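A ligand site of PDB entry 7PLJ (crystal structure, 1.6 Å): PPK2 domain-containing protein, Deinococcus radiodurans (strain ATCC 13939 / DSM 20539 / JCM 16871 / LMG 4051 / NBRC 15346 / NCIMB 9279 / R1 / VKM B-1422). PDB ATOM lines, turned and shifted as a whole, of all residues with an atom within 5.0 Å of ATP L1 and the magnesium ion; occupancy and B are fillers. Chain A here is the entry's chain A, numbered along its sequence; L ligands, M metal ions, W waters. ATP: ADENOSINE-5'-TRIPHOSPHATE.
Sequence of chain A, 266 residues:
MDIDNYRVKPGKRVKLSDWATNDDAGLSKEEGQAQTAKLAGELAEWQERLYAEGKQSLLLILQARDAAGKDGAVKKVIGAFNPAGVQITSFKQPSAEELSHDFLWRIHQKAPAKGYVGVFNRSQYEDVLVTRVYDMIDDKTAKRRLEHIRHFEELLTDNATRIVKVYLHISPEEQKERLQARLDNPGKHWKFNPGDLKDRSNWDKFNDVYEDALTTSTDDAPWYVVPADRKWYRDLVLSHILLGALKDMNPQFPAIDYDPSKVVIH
The side-chain hydroxyl (OG1) of Thr 131 lies within hydrogen-bond range of the backbone carbonyl oxygen (O) of Asp 127 (2.7 Å).
The guanidinium group (NH1) of Arg 182 lies within salt-bridge range of the side-chain carboxylate (OD2) of Asp 66.
NH1 of Arg 106 sits at hydrogen-bond distance from O of Lys 92 (2.8 Å).
O of Ala 64 lies within hydrogen-bond range of NZ of Lys 70, 2.9 Å away.
The side-chain amino group of Lys 70 is in hydrogen-bond range of the backbone carbonyl oxygen of Arg 65, 3.5 Å away.
The side-chain hydroxyl (OG) of Ser 90 is in hydrogen-bond range of the guanidinium group (NH1) of Arg 122 (2.8 Å).
O of Phe 91 sits at hydrogen-bond distance from NH1 of Arg 122 (3.0 Å).
The side-chain amino group of Lys 92 lies within salt-bridge range of an oxygen (O1A) of ATP L1.
NH2 of Arg 106 sits at hydrogen-bond distance from N7 of ATP L1 (3.1 Å).
The side-chain carboxylate (OE1) of Glu 126 lies within hydrogen-bond range of an oxygen (O2') of ATP L1 (2.7 Å).
The side-chain amino group of Lys 92 sits at hydrogen-bond distance from an oxygen (O3') of ATP L2 (3.3 Å).
O3G of ATP L2 lies within salt-bridge range of NZ of Lys 70 (2.6 Å).
The guanidinium group (NE) of Arg 122 lies within salt-bridge range of an oxygen (O2G) of ATP L1 (2.8 Å).
The guanidinium group (NH2) of Arg 182 is in salt-bridge range of an oxygen (O1A) of ATP L2, at 3.5 Å.
An oxygen (O1B) of ATP L2 is in salt-bridge range of the guanidinium group of Arg 122.
OE1 of Gln 93 lies close to O4' of ATP L1 (3.4 Å).
NZ of Lys 70 lies within salt-bridge range of O2G of ATP L1 (3.3 Å).
N of Lys 70 is in hydrogen-bond range of O3G of ATP L2 (2.8 Å).
The side-chain amide nitrogen (ND2) of Asn 193 lies within hydrogen-bond range of an oxygen (O1B) of ATP L1, at 3.3 Å.
The backbone NH (N) of Gln 93 sits at hydrogen-bond distance from an oxygen (O4') of ATP L1 (3.2 Å).
OD1 of Asp 127 is in hydrogen-bond range of N6 of ATP L1, at 2.9 Å.
OG of Ser 90 sits at hydrogen-bond distance from O2' of ATP L2, at 3.5 Å.
An oxygen (O1G) of ATP L2 sits close to the backbone NH (N) of Ala 67 (2.8 Å).
One residue has an atom within 4 Å of the magnesium ion: Asp 66.
The nearest printed residue that does not touch the magnesium ion is Ala 67 (4.03 Å).
O2B of ATP L1 is bound to the magnesium ion (2.0 Å).
The magnesium ion is bound by OD1 of Asp 66, 2.1 Å away.
The magnesium ion is bound by O1G of ATP L2 (2.1 Å).
An oxygen (O2A) of ATP L2 is bound to the magnesium ion, 2.1 Å away.
The magnesium ion is bound by an oxygen (O1G) of ATP L1 (2.1 Å).
O2B of ATP L2 binds the magnesium ion (2.2 Å).
The magnesium ion has six donor atoms within binding distance.
Water W5 bridges the side-chain carboxylate of Glu 126 (2.6 Å) and an oxygen (O2G) of ATP L1 (2.7 Å).
Water W1 lies within hydrogen-bond range of the guanidinium group (NH1) of Arg 182 (3.3 Å), the side-chain amide nitrogen (ND2) of Asn 193 (3.3 Å) and the side-chain carboxylate (OD2) of Asp 66 (3.4 Å).
Water W4 lies within hydrogen-bond range of OD2 of Asp 127 (2.7 Å), NH2 of Arg 106 (3.0 Å) and N6 of ATP L1 (3.1 Å).
Water W6 lies within hydrogen-bond range of OD1 of Asn 193 (3.0 Å) and O1B of ATP L1 (3.2 Å).
Water W3 bridges NE2 of Gln 93 (2.7 Å) and O5' of ATP L1 (3.3 Å).
O of Ala 64 touches O2G of ATP L1, 3.96 Å away.
O of Phe 91 touches C8 of ATP L1, at 3.6 Å.
Pro 94 touches ATP L1.
Val 130 touches ATP L1.
Hydrophobic or aromatic side chains that line ATP L1: Pro 94 and Val 130.
13 residues have an atom within 4 Å of ATP L1: Ala 64, Asp 66, Lys 70, Phe 91, Lys 92, Gln 93, Pro 94, Arg 106, Arg 122, Glu 126, Asp 127, Val 130 and Asn 193.
Along chain A the residues within 4 Å of ATP L1 span positions 64 to 193.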
ATOM      1  N   ALA A  64       2.175   4.978   9.098  1.00  0.00           N
ATOM      2  CA  ALA A  64       3.577   5.265   9.359  1.00  0.00           C
ATOM      3  C   ALA A  64       3.794   5.240  10.873  1.00  0.00           C
ATOM      4  O   ALA A  64       2.850   5.464  11.651  1.00  0.00           O
ATOM      5  CB  ALA A  64       4.018   6.625   8.800  1.00  0.00           C
ATOM      6  N   ARG A  65       5.022   4.908  11.272  1.00  0.00           N
ATOM      7  CA  ARG A  65       5.382   5.004  12.679  1.00  0.00           C
ATOM      8  C   ARG A  65       5.263   6.454  13.146  1.00  0.00           C
ATOM      9  O   ARG A  65       5.222   7.398  12.341  1.00  0.00           O
ATOM     10  CB  ARG A  65       6.812   4.526  12.929  1.00  0.00           C
ATOM     11  CG  ARG A  65       7.237   3.295  12.177  1.00  0.00           C
ATOM     12  CD  ARG A  65       7.061   2.097  12.987  1.00  0.00           C
ATOM     13  NE  ARG A  65       8.231   1.251  13.159  1.00  0.00           N
ATOM     14  CZ  ARG A  65       8.721   0.450  12.227  1.00  0.00           C
ATOM     15  NH1 ARG A  65       8.579   0.706  10.937  1.00  0.00           N
ATOM     16  NH2 ARG A  65       9.315  -0.685  12.594  1.00  0.00           N
ATOM     17  N   ASP A  66       5.214   6.628  14.457  1.00  0.00           N
ATOM     18  CA  ASP A  66       5.085   7.957  15.026  1.00  0.00           C
ATOM     19  C   ASP A  66       6.306   8.802  14.626  1.00  0.00           C
ATOM     20  O   ASP A  66       7.446   8.332  14.620  1.00  0.00           O
ATOM     21  CB  ASP A  66       4.950   7.858  16.556  1.00  0.00           C
ATOM     22  CG  ASP A  66       4.478   9.180  17.213  1.00  0.00           C
ATOM     23  OD1 ASP A  66       3.866  10.022  16.544  1.00  0.00           O
ATOM     24  OD2 ASP A  66       4.741   9.382  18.414  1.00  0.00           O
ATOM     25  N   ALA A  67       6.036  10.064  14.300  1.00  0.00           N
ATOM     26  CA  ALA A  67       6.963  11.077  13.831  1.00  0.00           C
ATOM     27  C   ALA A  67       7.403  10.860  12.389  1.00  0.00           C
ATOM     28  O   ALA A  67       8.245  11.612  11.906  1.00  0.00           O
ATOM     29  CB  ALA A  67       8.229  11.202  14.718  1.00  0.00           C
ATOM     30  N   LYS A  70       3.012  11.706   8.863  1.00  0.00           N
ATOM     31  CA  LYS A  70       1.610  11.705   8.420  1.00  0.00           C
ATOM     32  C   LYS A  70       1.019  13.103   8.558  1.00  0.00           C
ATOM     33  O   LYS A  70       0.418  13.653   7.616  1.00  0.00           O
ATOM     34  CB  LYS A  70       0.785  10.672   9.234  1.00  0.00           C
ATOM     35  CG  LYS A  70       1.297   9.198   9.084  1.00  0.00           C
ATOM     36  CD  LYS A  70       0.429   8.201   9.886  1.00  0.00           C
ATOM     37  CE  LYS A  70       0.475   8.439  11.419  1.00  0.00           C
ATOM     38  NZ  LYS A  70       1.853   8.195  11.982  1.00  0.00           N
ATOM     39  N   SER A  90      -8.624  11.272  11.283  1.00  0.00           N
ATOM     40  CA  SER A  90      -7.497  10.742  12.039  1.00  0.00           C
ATOM     41  C   SER A  90      -8.077   9.664  12.958  1.00  0.00           C
ATOM     42  O   SER A  90      -8.704   9.960  13.967  1.00  0.00           O
ATOM     43  CB  SER A  90      -6.812  11.869  12.817  1.00  0.00           C
ATOM     44  OG  SER A  90      -5.618  11.410  13.482  1.00  0.00           O
ATOM     45  N   PHE A  91      -7.883   8.399  12.581  1.00  0.00           N
ATOM     46  CA  PHE A  91      -8.473   7.292  13.314  1.00  0.00           C
ATOM     47  C   PHE A  91      -7.622   7.027  14.558  1.00  0.00           C
ATOM     48  O   PHE A  91      -6.402   6.820  14.459  1.00  0.00           O
ATOM     49  CB  PHE A  91      -8.551   6.032  12.446  1.00  0.00           C
ATOM     50  CG  PHE A  91      -9.724   6.049  11.491  1.00  0.00           C
ATOM     51  CD1 PHE A  91     -11.005   5.850  11.959  1.00  0.00           C
ATOM     52  CD2 PHE A  91      -9.528   6.219  10.120  1.00  0.00           C
ATOM     53  CE1 PHE A  91     -12.110   5.844  11.100  1.00  0.00           C
ATOM     54  CE2 PHE A  91     -10.633   6.217   9.238  1.00  0.00           C
ATOM     55  CZ  PHE A  91     -11.927   6.049   9.747  1.00  0.00           C
ATOM     56  N   LYS A  92      -8.260   7.093  15.719  1.00  0.00           N
ATOM     57  CA  LYS A  92      -7.623   6.883  17.012  1.00  0.00           C
ATOM     58  C   LYS A  92      -8.106   5.556  17.584  1.00  0.00           C
ATOM     59  O   LYS A  92      -8.731   4.771  16.881  1.00  0.00           O
ATOM     60  CB  LYS A  92      -7.925   8.076  17.918  1.00  0.00           C
ATOM     61  CG  LYS A  92      -7.561   9.337  17.166  1.00  0.00           C
ATOM     62  CD  LYS A  92      -7.283  10.516  18.026  1.00  0.00           C
ATOM     63  CE  LYS A  92      -7.019  11.714  17.143  1.00  0.00           C
ATOM     64  NZ  LYS A  92      -6.280  12.722  17.904  1.00  0.00           N
ATOM     65  N   GLN A  93      -7.771   5.307  18.853  1.00  0.00           N
ATOM     66  CA  GLN A  93      -8.194   4.086  19.532  1.00  0.00           C
ATOM     67  C   GLN A  93      -9.701   3.941  19.426  1.00  0.00           C
ATOM     68  O   GLN A  93     -10.425   4.913  19.730  1.00  0.00           O
ATOM     69  CB  GLN A  93      -7.788   4.128  21.018  1.00  0.00           C
ATOM     70  CG  GLN A  93      -6.257   4.235  21.222  1.00  0.00           C
ATOM     71  CD  GLN A  93      -5.717   5.698  21.348  1.00  0.00           C
ATOM     72  OE1 GLN A  93      -6.285   6.712  20.799  1.00  0.00           O
ATOM     73  NE2 GLN A  93      -4.581   5.809  22.049  1.00  0.00           N
ATOM     74  N   PRO A  94     -10.213   2.794  18.983  1.00  0.00           N
ATOM     75  CA  PRO A  94     -11.669   2.595  18.903  1.00  0.00           C
ATOM     76  C   PRO A  94     -12.371   2.893  20.212  1.00  0.00           C
ATOM     77  O   PRO A  94     -11.935   2.473  21.285  1.00  0.00           O
ATOM     78  CB  PRO A  94     -11.811   1.101  18.557  1.00  0.00           C
ATOM     79  CG  PRO A  94     -10.554   0.771  17.798  1.00  0.00           C
ATOM     80  CD  PRO A  94      -9.444   1.669  18.401  1.00  0.00           C
ATOM     81  N   ARG A 106     -16.585   1.510  11.507  1.00  0.00           N
ATOM     82  CA  ARG A 106     -16.210   2.914  11.634  1.00  0.00           C
ATOM     83  C   ARG A 106     -15.404   3.410  10.425  1.00  0.00           C
ATOM     84  O   ARG A 106     -15.394   4.623  10.143  1.00  0.00           O
ATOM     85  CB  ARG A 106     -15.418   3.110  12.927  1.00  0.00           C
ATOM     86  CG  ARG A 106     -13.959   2.581  12.861  1.00  0.00           C
ATOM     87  CD  ARG A 106     -13.197   2.920  14.182  1.00  0.00           C
ATOM     88  NE  ARG A 106     -11.762   2.621  14.086  1.00  0.00           N
ATOM     89  CZ  ARG A 106     -10.852   3.263  14.794  1.00  0.00           C
ATOM     90  NH1 ARG A 106     -11.173   4.253  15.628  1.00  0.00           N
ATOM     91  NH2 ARG A 106      -9.575   2.952  14.619  1.00  0.00           N
ATOM     92  N   ARG A 122      -4.073   7.057   9.466  1.00  0.00           N
ATOM     93  CA  ARG A 122      -4.353   5.729  10.020  1.00  0.00           C
ATOM     94  C   ARG A 122      -5.700   5.224   9.485  1.00  0.00           C
ATOM     95  O   ARG A 122      -6.471   6.000   8.911  1.00  0.00           O
ATOM     96  CB  ARG A 122      -4.330   5.725  11.550  1.00  0.00           C
ATOM     97  CG  ARG A 122      -3.047   6.326  12.127  1.00  0.00           C
ATOM     98  CD  ARG A 122      -3.161   6.309  13.661  1.00  0.00           C
ATOM     99  NE  ARG A 122      -2.503   7.502  14.163  1.00  0.00           N
ATOM    100  CZ  ARG A 122      -3.027   8.726  14.152  1.00  0.00           C
ATOM    101  NH1 ARG A 122      -4.322   8.937  13.994  1.00  0.00           N
ATOM    102  NH2 ARG A 122      -2.208   9.767  14.272  1.00  0.00           N
ATOM    103  N   GLU A 126      -4.699  -0.371  11.064  1.00  0.00           N
ATOM    104  CA  GLU A 126      -4.379  -0.412  12.504  1.00  0.00           C
ATOM    105  C   GLU A 126      -4.875  -1.698  13.143  1.00  0.00           C
ATOM    106  O   GLU A 126      -4.247  -2.221  14.073  1.00  0.00           O
ATOM    107  CB  GLU A 126      -5.000   0.789  13.223  1.00  0.00           C
ATOM    108  CG  GLU A 126      -4.445   2.136  12.755  1.00  0.00           C
ATOM    109  CD  GLU A 126      -3.164   2.486  13.522  1.00  0.00           C
ATOM    110  OE1 GLU A 126      -3.008   2.004  14.664  1.00  0.00           O
ATOM    111  OE2 GLU A 126      -2.306   3.220  13.000  1.00  0.00           O
ATOM    112  N   ASP A 127      -6.010  -2.229  12.654  1.00  0.00           N
ATOM    113  CA  ASP A 127      -6.556  -3.454  13.218  1.00  0.00           C
ATOM    114  C   ASP A 127      -5.730  -4.692  12.868  1.00  0.00           C
ATOM    115  O   ASP A 127      -6.059  -5.759  13.406  1.00  0.00           O
ATOM    116  CB  ASP A 127      -7.994  -3.611  12.740  1.00  0.00           C
ATOM    117  CG  ASP A 127      -8.909  -2.531  13.362  1.00  0.00           C
ATOM    118  OD1 ASP A 127      -9.110  -2.551  14.597  1.00  0.00           O
ATOM    119  OD2 ASP A 127      -9.351  -1.630  12.638  1.00  0.00           O
ATOM    120  N   VAL A 130      -0.827  -2.692  15.313  1.00  0.00           N
ATOM    121  CA  VAL A 130      -0.593  -2.674  16.764  1.00  0.00           C
ATOM    122  C   VAL A 130      -1.289  -3.847  17.444  1.00  0.00           C
ATOM    123  O   VAL A 130      -0.781  -4.392  18.426  1.00  0.00           O
ATOM    124  CB  VAL A 130      -1.031  -1.310  17.357  1.00  0.00           C
ATOM    125  CG1 VAL A 130      -2.539  -1.087  17.188  1.00  0.00           C
ATOM    126  CG2 VAL A 130      -0.629  -1.209  18.835  1.00  0.00           C
ATOM    127  N   THR A 131      -2.446  -4.269  16.920  1.00  0.00           N
ATOM    128  CA  THR A 131      -3.176  -5.384  17.526  1.00  0.00           C
ATOM    129  C   THR A 131      -2.394  -6.689  17.426  1.00  0.00           C
ATOM    130  O   THR A 131      -2.609  -7.588  18.233  1.00  0.00           O
ATOM    131  CB  THR A 131      -4.532  -5.536  16.844  1.00  0.00           C
ATOM    132  OG1 THR A 131      -4.344  -5.852  15.453  1.00  0.00           O
ATOM    133  CG2 THR A 131      -5.337  -4.220  16.986  1.00  0.00           C
ATOM    134  N   MET A 136      -3.198  -8.631  20.836  1.00  0.00           N
ATOM    135  CA  MET A 136      -4.628  -8.434  20.979  1.00  0.00           C
ATOM    136  C   MET A 136      -5.409  -9.355  20.056  1.00  0.00           C
ATOM    137  O   MET A 136      -6.546  -9.707  20.364  1.00  0.00           O
ATOM    138  CB  MET A 136      -4.994  -6.963  20.681  1.00  0.00           C
ATOM    139  CG  MET A 136      -4.204  -5.920  21.502  1.00  0.00           C
ATOM    140  SD  MET A 136      -4.439  -4.240  20.841  1.00  0.00           S
ATOM    141  CE  MET A 136      -6.225  -4.048  20.881  1.00  0.00           C
ATOM    142  N   ARG A 182      10.860  16.509  19.731  1.00  0.00           N
ATOM    143  CA  ARG A 182       9.643  16.738  20.514  1.00  0.00           C
ATOM    144  C   ARG A 182       9.960  16.960  21.979  1.00  0.00           C
ATOM    145  O   ARG A 182       9.376  17.844  22.624  1.00  0.00           O
ATOM    146  CB  ARG A 182       8.672  15.554  20.367  1.00  0.00           C
ATOM    147  CG  ARG A 182       8.125  15.405  18.990  1.00  0.00           C
ATOM    148  CD  ARG A 182       7.065  14.301  18.960  1.00  0.00           C
ATOM    149  NE  ARG A 182       6.528  14.140  17.611  1.00  0.00           N
ATOM    150  CZ  ARG A 182       5.752  13.122  17.244  1.00  0.00           C
ATOM    151  NH1 ARG A 182       5.407  12.163  18.089  1.00  0.00           N
ATOM    152  NH2 ARG A 182       5.273  13.097  15.998  1.00  0.00           N
ATOM    153  N   ASN A 193       4.675  10.386  23.851  1.00  0.00           N
ATOM    154  CA  ASN A 193       3.783   9.471  24.553  1.00  0.00           C
ATOM    155  C   ASN A 193       4.544   8.234  24.990  1.00  0.00           C
ATOM    156  O   ASN A 193       5.600   7.926  24.437  1.00  0.00           O
ATOM    157  CB  ASN A 193       2.549   9.078  23.694  1.00  0.00           C
ATOM    158  CG  ASN A 193       2.927   8.455  22.324  1.00  0.00           C
ATOM    159  OD1 ASN A 193       3.428   7.329  22.273  1.00  0.00           O
ATOM    160  ND2 ASN A 193       2.644   9.178  21.214  1.00  0.00           N
HETATM  161  PG  ATP L   1       1.015   7.309  15.387  1.00  0.00           P
HETATM  162  O1G ATP L   1       1.870   8.348  14.851  1.00  0.00           O
HETATM  163  O2G ATP L   1       0.150   6.607  14.313  1.00  0.00           O
HETATM  164  O3G ATP L   1       1.852   6.310  16.198  1.00  0.00           O
HETATM  165  PB  ATP L   1       0.087   9.045  17.530  1.00  0.00           P
HETATM  166  O1B ATP L   1       0.436   8.430  18.830  1.00  0.00           O
HETATM  167  O2B ATP L   1       1.009  10.109  16.966  1.00  0.00           O
HETATM  168  O3B ATP L   1       0.039   7.934  16.404  1.00  0.00           O
HETATM  169  PA  ATP L   1      -2.535   9.723  18.583  1.00  0.00           P
HETATM  170  O1A ATP L   1      -3.696  10.358  17.923  1.00  0.00           O
HETATM  171  O2A ATP L   1      -1.965  10.343  19.818  1.00  0.00           O
HETATM  172  O3A ATP L   1      -1.389   9.626  17.546  1.00  0.00           O
HETATM  173  O5' ATP L   1      -2.814   8.210  18.921  1.00  0.00           O
HETATM  174  C5' ATP L   1      -3.823   7.473  18.210  1.00  0.00           C
HETATM  175  C4' ATP L   1      -3.567   6.050  18.571  1.00  0.00           C
HETATM  176  O4' ATP L   1      -4.692   5.225  18.167  1.00  0.00           O
HETATM  177  C3' ATP L   1      -2.326   5.446  17.920  1.00  0.00           C
HETATM  178  O3' ATP L   1      -1.485   4.860  18.911  1.00  0.00           O
HETATM  179  C2' ATP L   1      -2.905   4.329  17.035  1.00  0.00           C
HETATM  180  O2' ATP L   1      -1.990   3.248  16.871  1.00  0.00           O
HETATM  181  C1' ATP L   1      -4.147   3.976  17.836  1.00  0.00           C
HETATM  182  N9  ATP L   1      -5.122   3.231  17.051  1.00  0.00           N
HETATM  183  C8  ATP L   1      -5.736   3.627  15.896  1.00  0.00           C
HETATM  184  N7  ATP L   1      -6.534   2.713  15.383  1.00  0.00           N
HETATM  185  C5  ATP L   1      -6.421   1.642  16.257  1.00  0.00           C
HETATM  186  C6  ATP L   1      -7.003   0.357  16.276  1.00  0.00           C
HETATM  187  N6  ATP L   1      -7.849  -0.094  15.346  1.00  0.00           N
HETATM  188  N1  ATP L   1      -6.686  -0.466  17.302  1.00  0.00           N
HETATM  189  C2  ATP L   1      -5.841  -0.023  18.243  1.00  0.00           C
HETATM  190  N3  ATP L   1      -5.208   1.158  18.301  1.00  0.00           N
HETATM  191  C4  ATP L   1      -5.558   1.946  17.291  1.00  0.00           C
HETATM  192  PG  ATP L   2       3.358  11.364  12.429  1.00  0.00           P
HETATM  193  O1G ATP L   2       3.430  10.771  13.764  1.00  0.00           O
HETATM  194  O2G ATP L   2       4.409  12.397  12.115  1.00  0.00           O
HETATM  195  O3G ATP L   2       3.250  10.342  11.339  1.00  0.00           O
HETATM  196  PB  ATP L   2       0.583  12.122  13.161  1.00  0.00           P
HETATM  197  O1B ATP L   2      -0.598  12.312  12.214  1.00  0.00           O
HETATM  198  O2B ATP L   2       0.565  10.887  14.038  1.00  0.00           O
HETATM  199  O3B ATP L   2       1.935  12.143  12.380  1.00  0.00           O
HETATM  200  PA  ATP L   2       1.592  13.678  15.458  1.00  0.00           P
HETATM  201  O1A ATP L   2       2.364  14.891  15.132  1.00  0.00           O
HETATM  202  O2A ATP L   2       2.230  12.428  15.892  1.00  0.00           O
HETATM  203  O3A ATP L   2       0.776  13.369  14.120  1.00  0.00           O
HETATM  204  O5' ATP L   2       0.437  14.170  16.408  1.00  0.00           O
HETATM  205  C5' ATP L   2      -0.141  13.307  17.424  1.00  0.00           C
HETATM  206  C4' ATP L   2      -1.659  13.310  17.297  1.00  0.00           C
HETATM  207  O4' ATP L   2      -2.193  14.644  17.480  1.00  0.00           O
HETATM  208  C3' ATP L   2      -2.206  12.825  15.955  1.00  0.00           C
HETATM  209  O3' ATP L   2      -3.473  12.221  16.171  1.00  0.00           O
HETATM  210  C2' ATP L   2      -2.389  14.127  15.182  1.00  0.00           C
HETATM  211  O2' ATP L   2      -3.381  14.001  14.169  1.00  0.00           O
HETATM  212  C1' ATP L   2      -2.843  15.077  16.297  1.00  0.00           C
HETATM  213  N9  ATP L   2      -2.439  16.477  16.082  1.00  0.00           N
HETATM  214  C8  ATP L   2      -1.138  16.932  16.068  1.00  0.00           C
HETATM  215  N7  ATP L   2      -1.037  18.231  15.915  1.00  0.00           N
HETATM  216  C5  ATP L   2      -2.352  18.654  15.795  1.00  0.00           C
HETATM  217  C6  ATP L   2      -2.923  19.932  15.606  1.00  0.00           C
HETATM  218  N6  ATP L   2      -2.192  21.050  15.471  1.00  0.00           N
HETATM  219  N1  ATP L   2      -4.273  20.020  15.545  1.00  0.00           N
HETATM  220  C2  ATP L   2      -4.992  18.897  15.658  1.00  0.00           C
HETATM  221  N3  ATP L   2      -4.565  17.642  15.852  1.00  0.00           N
HETATM  222  C4  ATP L   2      -3.228  17.588  15.894  1.00  0.00           C
HETATM  223 MG    MG M   1       2.167  10.392  15.391  1.00  0.00          MG
HETATM  224  O   HOH W   1       2.320  11.658  19.054  1.00  0.00           O
HETATM  225  O   HOH W   2      -3.285   1.238  20.369  1.00  0.00           O
HETATM  226  O   HOH W   3      -3.123   8.118  22.169  1.00  0.00           O
HETATM  227  O   HOH W   4      -8.652   0.990  12.550  1.00  0.00           O
HETATM  228  O   HOH W   5       0.002   4.015  13.754  1.00  0.00           O
HETATM  229  O   HOH W   6       2.747   6.364  19.552  1.00  0.00           O
HETATM  230  O   HOH W   7      -0.855   2.034  19.443  1.00  0.00           O
HETATM  231  O   HOH W   8      -0.515   6.660  20.550  1.00  0.00           O
HETATM  232  O   HOH W   9       0.059  11.774  20.692  1.00  0.00           O
HETATM  233  O   HOH W  10       0.972   4.349  17.343  1.00  0.00           O
HETATM  234  O   HOH W  11      -8.484  -2.466  18.354  1.00  0.00           O
